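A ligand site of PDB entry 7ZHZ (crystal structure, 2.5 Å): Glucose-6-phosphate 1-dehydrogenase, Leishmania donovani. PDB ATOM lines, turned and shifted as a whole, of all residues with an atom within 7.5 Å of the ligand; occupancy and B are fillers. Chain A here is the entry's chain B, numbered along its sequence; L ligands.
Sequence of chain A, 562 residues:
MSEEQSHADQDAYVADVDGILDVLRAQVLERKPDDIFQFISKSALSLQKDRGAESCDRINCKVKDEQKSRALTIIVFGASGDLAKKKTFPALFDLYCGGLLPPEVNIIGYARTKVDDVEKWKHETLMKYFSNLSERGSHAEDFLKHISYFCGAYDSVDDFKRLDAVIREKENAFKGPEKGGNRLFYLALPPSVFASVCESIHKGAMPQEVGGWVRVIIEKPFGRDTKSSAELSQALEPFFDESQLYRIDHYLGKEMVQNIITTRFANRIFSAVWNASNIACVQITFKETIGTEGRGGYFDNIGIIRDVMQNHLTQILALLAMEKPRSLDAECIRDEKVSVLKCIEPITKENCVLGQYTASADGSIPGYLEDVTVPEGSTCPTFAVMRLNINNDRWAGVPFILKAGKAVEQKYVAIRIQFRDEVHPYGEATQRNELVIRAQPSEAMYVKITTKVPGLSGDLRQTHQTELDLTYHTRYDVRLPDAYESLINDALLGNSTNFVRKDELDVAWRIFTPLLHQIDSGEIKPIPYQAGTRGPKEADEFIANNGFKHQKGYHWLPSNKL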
ATOM      1  N   LYS A  87      -0.617  16.707  19.036  1.00  0.00           N
ATOM      2  CA  LYS A  87      -1.349  17.766  18.365  1.00  0.00           C
ATOM      3  C   LYS A  87      -0.590  18.374  17.197  1.00  0.00           C
ATOM      4  O   LYS A  87      -1.213  18.804  16.220  1.00  0.00           O
ATOM      5  CB  LYS A  87      -1.746  18.856  19.357  1.00  0.00           C
ATOM      6  CG  LYS A  87      -2.730  19.870  18.794  1.00  0.00           C
ATOM      7  CD  LYS A  87      -4.111  19.736  19.411  1.00  0.00           C
ATOM      8  CE  LYS A  87      -5.208  19.975  18.378  1.00  0.00           C
ATOM      9  NZ  LYS A  87      -6.475  19.258  18.716  1.00  0.00           N
ATOM     10  N   HIS A 250      -4.183  28.575  20.672  1.00  0.00           N
ATOM     11  CA  HIS A 250      -5.048  27.658  19.945  1.00  0.00           C
ATOM     12  C   HIS A 250      -6.517  27.972  20.116  1.00  0.00           C
ATOM     13  O   HIS A 250      -7.370  27.119  19.869  1.00  0.00           O
ATOM     14  CB  HIS A 250      -4.768  26.210  20.358  1.00  0.00           C
ATOM     15  CG  HIS A 250      -5.070  25.911  21.800  1.00  0.00           C
ATOM     16  ND1 HIS A 250      -4.215  26.253  22.820  1.00  0.00           N
ATOM     17  CD2 HIS A 250      -6.125  25.280  22.373  1.00  0.00           C
ATOM     18  CE1 HIS A 250      -4.737  25.863  23.968  1.00  0.00           C
ATOM     19  NE2 HIS A 250      -5.893  25.266  23.726  1.00  0.00           N
ATOM     20  N   TYR A 251      -6.836  29.186  20.559  1.00  0.00           N
ATOM     21  CA  TYR A 251      -8.201  29.683  20.514  1.00  0.00           C
ATOM     22  C   TYR A 251      -8.431  30.732  19.442  1.00  0.00           C
ATOM     23  O   TYR A 251      -9.584  30.964  19.081  1.00  0.00           O
ATOM     24  CB  TYR A 251      -8.614  30.259  21.876  1.00  0.00           C
ATOM     25  CG  TYR A 251      -9.102  29.190  22.813  1.00  0.00           C
ATOM     26  CD1 TYR A 251      -8.247  28.201  23.263  1.00  0.00           C
ATOM     27  CD2 TYR A 251     -10.426  29.151  23.216  1.00  0.00           C
ATOM     28  CE1 TYR A 251      -8.684  27.214  24.119  1.00  0.00           C
ATOM     29  CE2 TYR A 251     -10.884  28.160  24.069  1.00  0.00           C
ATOM     30  CZ  TYR A 251     -10.000  27.193  24.510  1.00  0.00           C
ATOM     31  OH  TYR A 251     -10.429  26.200  25.356  1.00  0.00           O
ATOM     32  N   GLY A 253      -7.348  30.616  16.300  1.00  0.00           N
ATOM     33  CA  GLY A 253      -7.697  29.932  15.069  1.00  0.00           C
ATOM     34  C   GLY A 253      -9.083  29.318  15.095  1.00  0.00           C
ATOM     35  O   GLY A 253      -9.474  28.642  14.138  1.00  0.00           O
ATOM     36  N   LYS A 254      -9.827  29.542  16.180  1.00  0.00           N
ATOM     37  CA  LYS A 254     -11.159  28.975  16.303  1.00  0.00           C
ATOM     38  C   LYS A 254     -12.081  29.523  15.227  1.00  0.00           C
ATOM     39  O   LYS A 254     -11.939  30.657  14.780  1.00  0.00           O
ATOM     40  CB  LYS A 254     -11.744  29.273  17.685  1.00  0.00           C
ATOM     41  CG  LYS A 254     -11.355  28.295  18.767  1.00  0.00           C
ATOM     42  CD  LYS A 254     -11.791  26.895  18.433  1.00  0.00           C
ATOM     43  CE  LYS A 254     -12.479  26.292  19.639  1.00  0.00           C
ATOM     44  NZ  LYS A 254     -12.482  24.821  19.633  1.00  0.00           N
ATOM     45  N   GLU A 255     -13.042  28.695  14.817  1.00  0.00           N
ATOM     46  CA  GLU A 255     -13.991  29.111  13.788  1.00  0.00           C
ATOM     47  C   GLU A 255     -14.818  30.307  14.249  1.00  0.00           C
ATOM     48  O   GLU A 255     -15.062  31.234  13.472  1.00  0.00           O
ATOM     49  CB  GLU A 255     -14.891  27.947  13.394  1.00  0.00           C
ATOM     50  CG  GLU A 255     -14.323  27.075  12.299  1.00  0.00           C
ATOM     51  CD  GLU A 255     -14.715  27.551  10.928  1.00  0.00           C
ATOM     52  OE1 GLU A 255     -15.887  27.943  10.763  1.00  0.00           O
ATOM     53  OE2 GLU A 255     -13.858  27.537  10.021  1.00  0.00           O
ATOM     54  N   PHE A 286     -15.518  29.959  30.772  1.00  0.00           N
ATOM     55  CA  PHE A 286     -14.749  28.756  30.450  1.00  0.00           C
ATOM     56  C   PHE A 286     -15.038  27.716  31.520  1.00  0.00           C
ATOM     57  O   PHE A 286     -14.724  27.931  32.703  1.00  0.00           O
ATOM     58  CB  PHE A 286     -13.261  29.064  30.379  1.00  0.00           C
ATOM     59  CG  PHE A 286     -12.421  27.928  29.877  1.00  0.00           C
ATOM     60  CD1 PHE A 286     -11.923  26.972  30.744  1.00  0.00           C
ATOM     61  CD2 PHE A 286     -12.128  27.816  28.524  1.00  0.00           C
ATOM     62  CE1 PHE A 286     -11.157  25.925  30.277  1.00  0.00           C
ATOM     63  CE2 PHE A 286     -11.370  26.769  28.051  1.00  0.00           C
ATOM     64  CZ  PHE A 286     -10.880  25.818  28.928  1.00  0.00           C
ATOM     65  N   GLU A 288     -15.064  23.403  32.606  1.00  0.00           N
ATOM     66  CA  GLU A 288     -14.553  22.063  32.370  1.00  0.00           C
ATOM     67  C   GLU A 288     -15.054  21.135  33.460  1.00  0.00           C
ATOM     68  O   GLU A 288     -14.951  21.456  34.647  1.00  0.00           O
ATOM     69  CB  GLU A 288     -13.025  22.036  32.328  1.00  0.00           C
ATOM     70  CG  GLU A 288     -12.409  22.654  31.084  1.00  0.00           C
ATOM     71  CD  GLU A 288     -11.015  22.124  30.821  1.00  0.00           C
ATOM     72  OE1 GLU A 288     -10.090  22.455  31.596  1.00  0.00           O
ATOM     73  OE2 GLU A 288     -10.836  21.378  29.830  1.00  0.00           O
ATOM     74  N   HIS A 312      -6.433  33.098  27.174  1.00  0.00           N
ATOM     75  CA  HIS A 312      -7.543  32.770  26.278  1.00  0.00           C
ATOM     76  C   HIS A 312      -8.657  33.807  26.369  1.00  0.00           C
ATOM     77  O   HIS A 312      -8.998  34.455  25.375  1.00  0.00           O
ATOM     78  CB  HIS A 312      -8.080  31.371  26.592  1.00  0.00           C
ATOM     79  CG  HIS A 312      -7.139  30.259  26.260  1.00  0.00           C
ATOM     80  ND1 HIS A 312      -6.305  30.293  25.154  1.00  0.00           N
ATOM     81  CD2 HIS A 312      -6.888  29.082  26.880  1.00  0.00           C
ATOM     82  CE1 HIS A 312      -5.586  29.180  25.116  1.00  0.00           C
ATOM     83  NE2 HIS A 312      -5.925  28.429  26.154  1.00  0.00           N
ATOM     84  N   LYS A 411     -19.098  21.104  30.567  1.00  0.00           N
ATOM     85  CA  LYS A 411     -18.055  21.645  29.695  1.00  0.00           C
ATOM     86  C   LYS A 411     -18.685  22.690  28.786  1.00  0.00           C
ATOM     87  O   LYS A 411     -19.659  22.409  28.081  1.00  0.00           O
ATOM     88  CB  LYS A 411     -17.408  20.532  28.871  1.00  0.00           C
ATOM     89  CG  LYS A 411     -16.189  20.983  28.083  1.00  0.00           C
ATOM     90  CD  LYS A 411     -15.626  19.860  27.224  1.00  0.00           C
ATOM     91  CE  LYS A 411     -14.331  20.286  26.539  1.00  0.00           C
ATOM     92  NZ  LYS A 411     -13.713  19.178  25.775  1.00  0.00           N
ATOM     93  N   VAL A 413     -17.700  26.660  26.749  1.00  0.00           N
ATOM     94  CA  VAL A 413     -16.903  27.833  26.404  1.00  0.00           C
ATOM     95  C   VAL A 413     -17.782  28.719  25.549  1.00  0.00           C
ATOM     96  O   VAL A 413     -18.071  28.385  24.389  1.00  0.00           O
ATOM     97  CB  VAL A 413     -15.604  27.465  25.666  1.00  0.00           C
ATOM     98  CG1 VAL A 413     -14.871  28.726  25.232  1.00  0.00           C
ATOM     99  CG2 VAL A 413     -14.719  26.588  26.529  1.00  0.00           C
ATOM    100  N   ALA A 439     -18.393  27.990  21.426  1.00  0.00           N
ATOM    101  CA  ALA A 439     -17.333  27.359  20.645  1.00  0.00           C
ATOM    102  C   ALA A 439     -17.037  25.933  21.068  1.00  0.00           C
ATOM    103  O   ALA A 439     -16.467  25.182  20.268  1.00  0.00           O
ATOM    104  CB  ALA A 439     -16.038  28.180  20.741  1.00  0.00           C
ATOM    105  N   GLN A 440     -17.404  25.538  22.290  1.00  0.00           N
ATOM    106  CA  GLN A 440     -17.163  24.196  22.808  1.00  0.00           C
ATOM    107  C   GLN A 440     -18.302  23.892  23.773  1.00  0.00           C
ATOM    108  O   GLN A 440     -18.661  24.761  24.576  1.00  0.00           O
ATOM    109  CB  GLN A 440     -15.807  24.095  23.523  1.00  0.00           C
ATOM    110  CG  GLN A 440     -15.450  22.710  24.032  1.00  0.00           C
ATOM    111  CD  GLN A 440     -14.699  21.885  23.004  1.00  0.00           C
ATOM    112  OE1 GLN A 440     -15.168  20.833  22.575  1.00  0.00           O
ATOM    113  NE2 GLN A 440     -13.522  22.358  22.615  1.00  0.00           N
ATOM    114  N   PRO A 441     -18.883  22.673  23.731  1.00  0.00           N
ATOM    115  CA  PRO A 441     -18.526  21.523  22.891  1.00  0.00           C
ATOM    116  C   PRO A 441     -18.923  21.674  21.420  1.00  0.00           C
ATOM    117  O   PRO A 441     -18.227  21.153  20.545  1.00  0.00           O
ATOM    118  CB  PRO A 441     -19.298  20.378  23.538  1.00  0.00           C
ATOM    119  CG  PRO A 441     -20.477  21.021  24.155  1.00  0.00           C
ATOM    120  CD  PRO A 441     -20.020  22.373  24.621  1.00  0.00           C
ATOM    121  N   SER A 442     -20.030  22.356  21.144  1.00  0.00           N
ATOM    122  CA  SER A 442     -20.523  22.562  19.792  1.00  0.00           C
ATOM    123  C   SER A 442     -20.588  24.057  19.505  1.00  0.00           C
ATOM    124  O   SER A 442     -21.138  24.822  20.312  1.00  0.00           O
ATOM    125  CB  SER A 442     -21.898  21.917  19.589  1.00  0.00           C
ATOM    126  OG  SER A 442     -22.011  20.724  20.337  1.00  0.00           O
ATOM    127  N   GLU A 443     -20.040  24.470  18.373  1.00  0.00           N
ATOM    128  CA  GLU A 443     -20.078  25.882  17.997  1.00  0.00           C
ATOM    129  C   GLU A 443     -21.501  26.285  17.633  1.00  0.00           C
ATOM    130  O   GLU A 443     -22.211  25.561  16.935  1.00  0.00           O
ATOM    131  CB  GLU A 443     -19.127  26.160  16.830  1.00  0.00           C
ATOM    132  CG  GLU A 443     -19.173  25.113  15.723  1.00  0.00           C
ATOM    133  CD  GLU A 443     -18.471  25.594  14.467  1.00  0.00           C
ATOM    134  OE1 GLU A 443     -18.281  26.818  14.318  1.00  0.00           O
ATOM    135  OE2 GLU A 443     -18.109  24.740  13.621  1.00  0.00           O
ATOM    136  N   LEU A 480     -13.626  19.578   8.745  1.00  0.00           N
ATOM    137  CA  LEU A 480     -13.638  20.055  10.127  1.00  0.00           C
ATOM    138  C   LEU A 480     -12.219  20.107  10.688  1.00  0.00           C
ATOM    139  O   LEU A 480     -11.798  19.209  11.416  1.00  0.00           O
ATOM    140  CB  LEU A 480     -14.519  19.156  10.993  1.00  0.00           C
ATOM    141  CG  LEU A 480     -14.786  19.593  12.434  1.00  0.00           C
ATOM    142  CD1 LEU A 480     -15.282  21.030  12.482  1.00  0.00           C
ATOM    143  CD2 LEU A 480     -15.776  18.654  13.105  1.00  0.00           C
ATOM    144  N   PRO A 481     -11.473  21.150  10.336  1.00  0.00           N
ATOM    145  CA  PRO A 481     -10.122  21.318  10.883  1.00  0.00           C
ATOM    146  C   PRO A 481     -10.169  21.813  12.317  1.00  0.00           C
ATOM    147  O   PRO A 481     -11.158  22.393  12.782  1.00  0.00           O
ATOM    148  CB  PRO A 481      -9.495  22.355   9.957  1.00  0.00           C
ATOM    149  CG  PRO A 481     -10.652  23.182   9.499  1.00  0.00           C
ATOM    150  CD  PRO A 481     -11.854  22.273   9.448  1.00  0.00           C
ATOM    151  N   ASP A 482      -9.068  21.585  13.022  1.00  0.00           N
ATOM    152  CA  ASP A 482      -8.957  22.090  14.383  1.00  0.00           C
ATOM    153  C   ASP A 482      -8.305  23.470  14.382  1.00  0.00           C
ATOM    154  O   ASP A 482      -7.866  23.973  13.352  1.00  0.00           O
ATOM    155  CB  ASP A 482      -8.184  21.095  15.256  1.00  0.00           C
ATOM    156  CG  ASP A 482      -6.683  21.280  15.172  1.00  0.00           C
ATOM    157  OD1 ASP A 482      -6.154  22.143  15.897  1.00  0.00           O
ATOM    158  OD2 ASP A 482      -6.037  20.539  14.401  1.00  0.00           O
ATOM    159  N   ALA A 483      -8.272  24.089  15.567  1.00  0.00           N
ATOM    160  CA  ALA A 483      -7.808  25.475  15.665  1.00  0.00           C
ATOM    161  C   ALA A 483      -6.349  25.605  15.254  1.00  0.00           C
ATOM    162  O   ALA A 483      -5.970  26.601  14.623  1.00  0.00           O
ATOM    163  CB  ALA A 483      -8.014  25.989  17.081  1.00  0.00           C
ATOM    164  N   TYR A 484      -5.513  24.623  15.605  1.00  0.00           N
ATOM    165  CA  TYR A 484      -4.116  24.670  15.201  1.00  0.00           C
ATOM    166  C   TYR A 484      -3.981  24.796  13.693  1.00  0.00           C
ATOM    167  O   TYR A 484      -3.311  25.694  13.193  1.00  0.00           O
ATOM    168  CB  TYR A 484      -3.380  23.431  15.696  1.00  0.00           C
ATOM    169  CG  TYR A 484      -2.934  23.497  17.138  1.00  0.00           C
ATOM    170  CD1 TYR A 484      -1.626  23.843  17.473  1.00  0.00           C
ATOM    171  CD2 TYR A 484      -3.818  23.204  18.172  1.00  0.00           C
ATOM    172  CE1 TYR A 484      -1.218  23.897  18.793  1.00  0.00           C
ATOM    173  CE2 TYR A 484      -3.410  23.257  19.493  1.00  0.00           C
ATOM    174  CZ  TYR A 484      -2.117  23.610  19.795  1.00  0.00           C
ATOM    175  OH  TYR A 484      -1.717  23.663  21.110  1.00  0.00           O
ATOM    176  N   GLU A 485      -4.666  23.920  12.949  1.00  0.00           N
ATOM    177  CA  GLU A 485      -4.427  23.799  11.516  1.00  0.00           C
ATOM    178  C   GLU A 485      -4.627  25.114  10.779  1.00  0.00           C
ATOM    179  O   GLU A 485      -4.044  25.292   9.696  1.00  0.00           O
ATOM    180  CB  GLU A 485      -5.332  22.719  10.928  1.00  0.00           C
ATOM    181  CG  GLU A 485      -5.084  21.337  11.509  1.00  0.00           C
ATOM    182  CD  GLU A 485      -6.124  20.326  11.100  1.00  0.00           C
ATOM    183  OE1 GLU A 485      -6.831  20.558  10.099  1.00  0.00           O
ATOM    184  OE2 GLU A 485      -6.242  19.291  11.792  1.00  0.00           O
ATOM    185  N   SER A 486      -5.424  26.033  11.317  1.00  0.00           N
ATOM    186  CA  SER A 486      -5.390  27.400  10.838  1.00  0.00           C
ATOM    187  C   SER A 486      -4.077  28.085  11.201  1.00  0.00           C
ATOM    188  O   SER A 486      -3.463  28.752  10.368  1.00  0.00           O
ATOM    189  CB  SER A 486      -6.579  28.192  11.391  1.00  0.00           C
ATOM    190  OG  SER A 486      -7.729  27.371  11.509  1.00  0.00           O
HETATM  191  C1  LIG L   1     -12.956  21.623  18.773  1.00  0.00           C
HETATM  192  C2  LIG L   1     -12.663  22.391  17.479  1.00  0.00           C
HETATM  193  O1  LIG L   1     -14.275  21.788  19.086  1.00  0.00           O
HETATM  194  O2  LIG L   1     -12.130  22.123  19.916  1.00  0.00           O
HETATM  195  C3  LIG L   1     -11.208  22.510  17.164  1.00  0.00           C
HETATM  196  O3  LIG L   1     -13.316  21.722  16.392  1.00  0.00           O
HETATM  197  C4  LIG L   1     -10.320  22.823  18.333  1.00  0.00           C
HETATM  198  O4  LIG L   1     -11.069  23.584  16.206  1.00  0.00           O
HETATM  199  C5  LIG L   1     -10.680  22.079  19.633  1.00  0.00           C
HETATM  200  O5  LIG L   1      -8.944  22.529  17.994  1.00  0.00           O
HETATM  201  C6  LIG L   1      -9.943  22.730  20.741  1.00  0.00           C
HETATM  202  O6  LIG L   1     -10.525  22.368  21.992  1.00  0.00           O
HETATM  203  P1  LIG L   1      -9.516  22.241  23.309  1.00  0.00           P
HETATM  204  O7  LIG L   1     -10.188  21.426  24.380  1.00  0.00           O
HETATM  205  O8  LIG L   1      -9.213  23.618  23.842  1.00  0.00           O
HETATM  206  O9  LIG L   1      -8.243  21.566  22.894  1.00  0.00           O
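The backbone carbonyl oxygen (O) of Gln 440 lies within hydrogen-bond range of the backbone NH (N) of Val 413 (3.0 Å). OD1 of Asp 482 is in hydrogen-bond range of N of Tyr 484 (2.6 Å).
Merely in contact with the ligand: Asp 482, Pro 481 and His 250. Hydrophobic or aromatic side chains within 4 Å of the ligand: His 250, Tyr 251 and Ala 483.
NZ of Lys 254 is in hydrogen-bond range of O2 of the ligand (2.7 Å). N of Ala 483 is in hydrogen-bond range of O4 of the ligand, 2.9 Å away. O2 of the ligand is in hydrogen-bond range of NE2 of Gln 440 (3.0 Å). OH of Tyr 251 lies within hydrogen-bond range of O8 of the ligand, 3.2 Å away.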
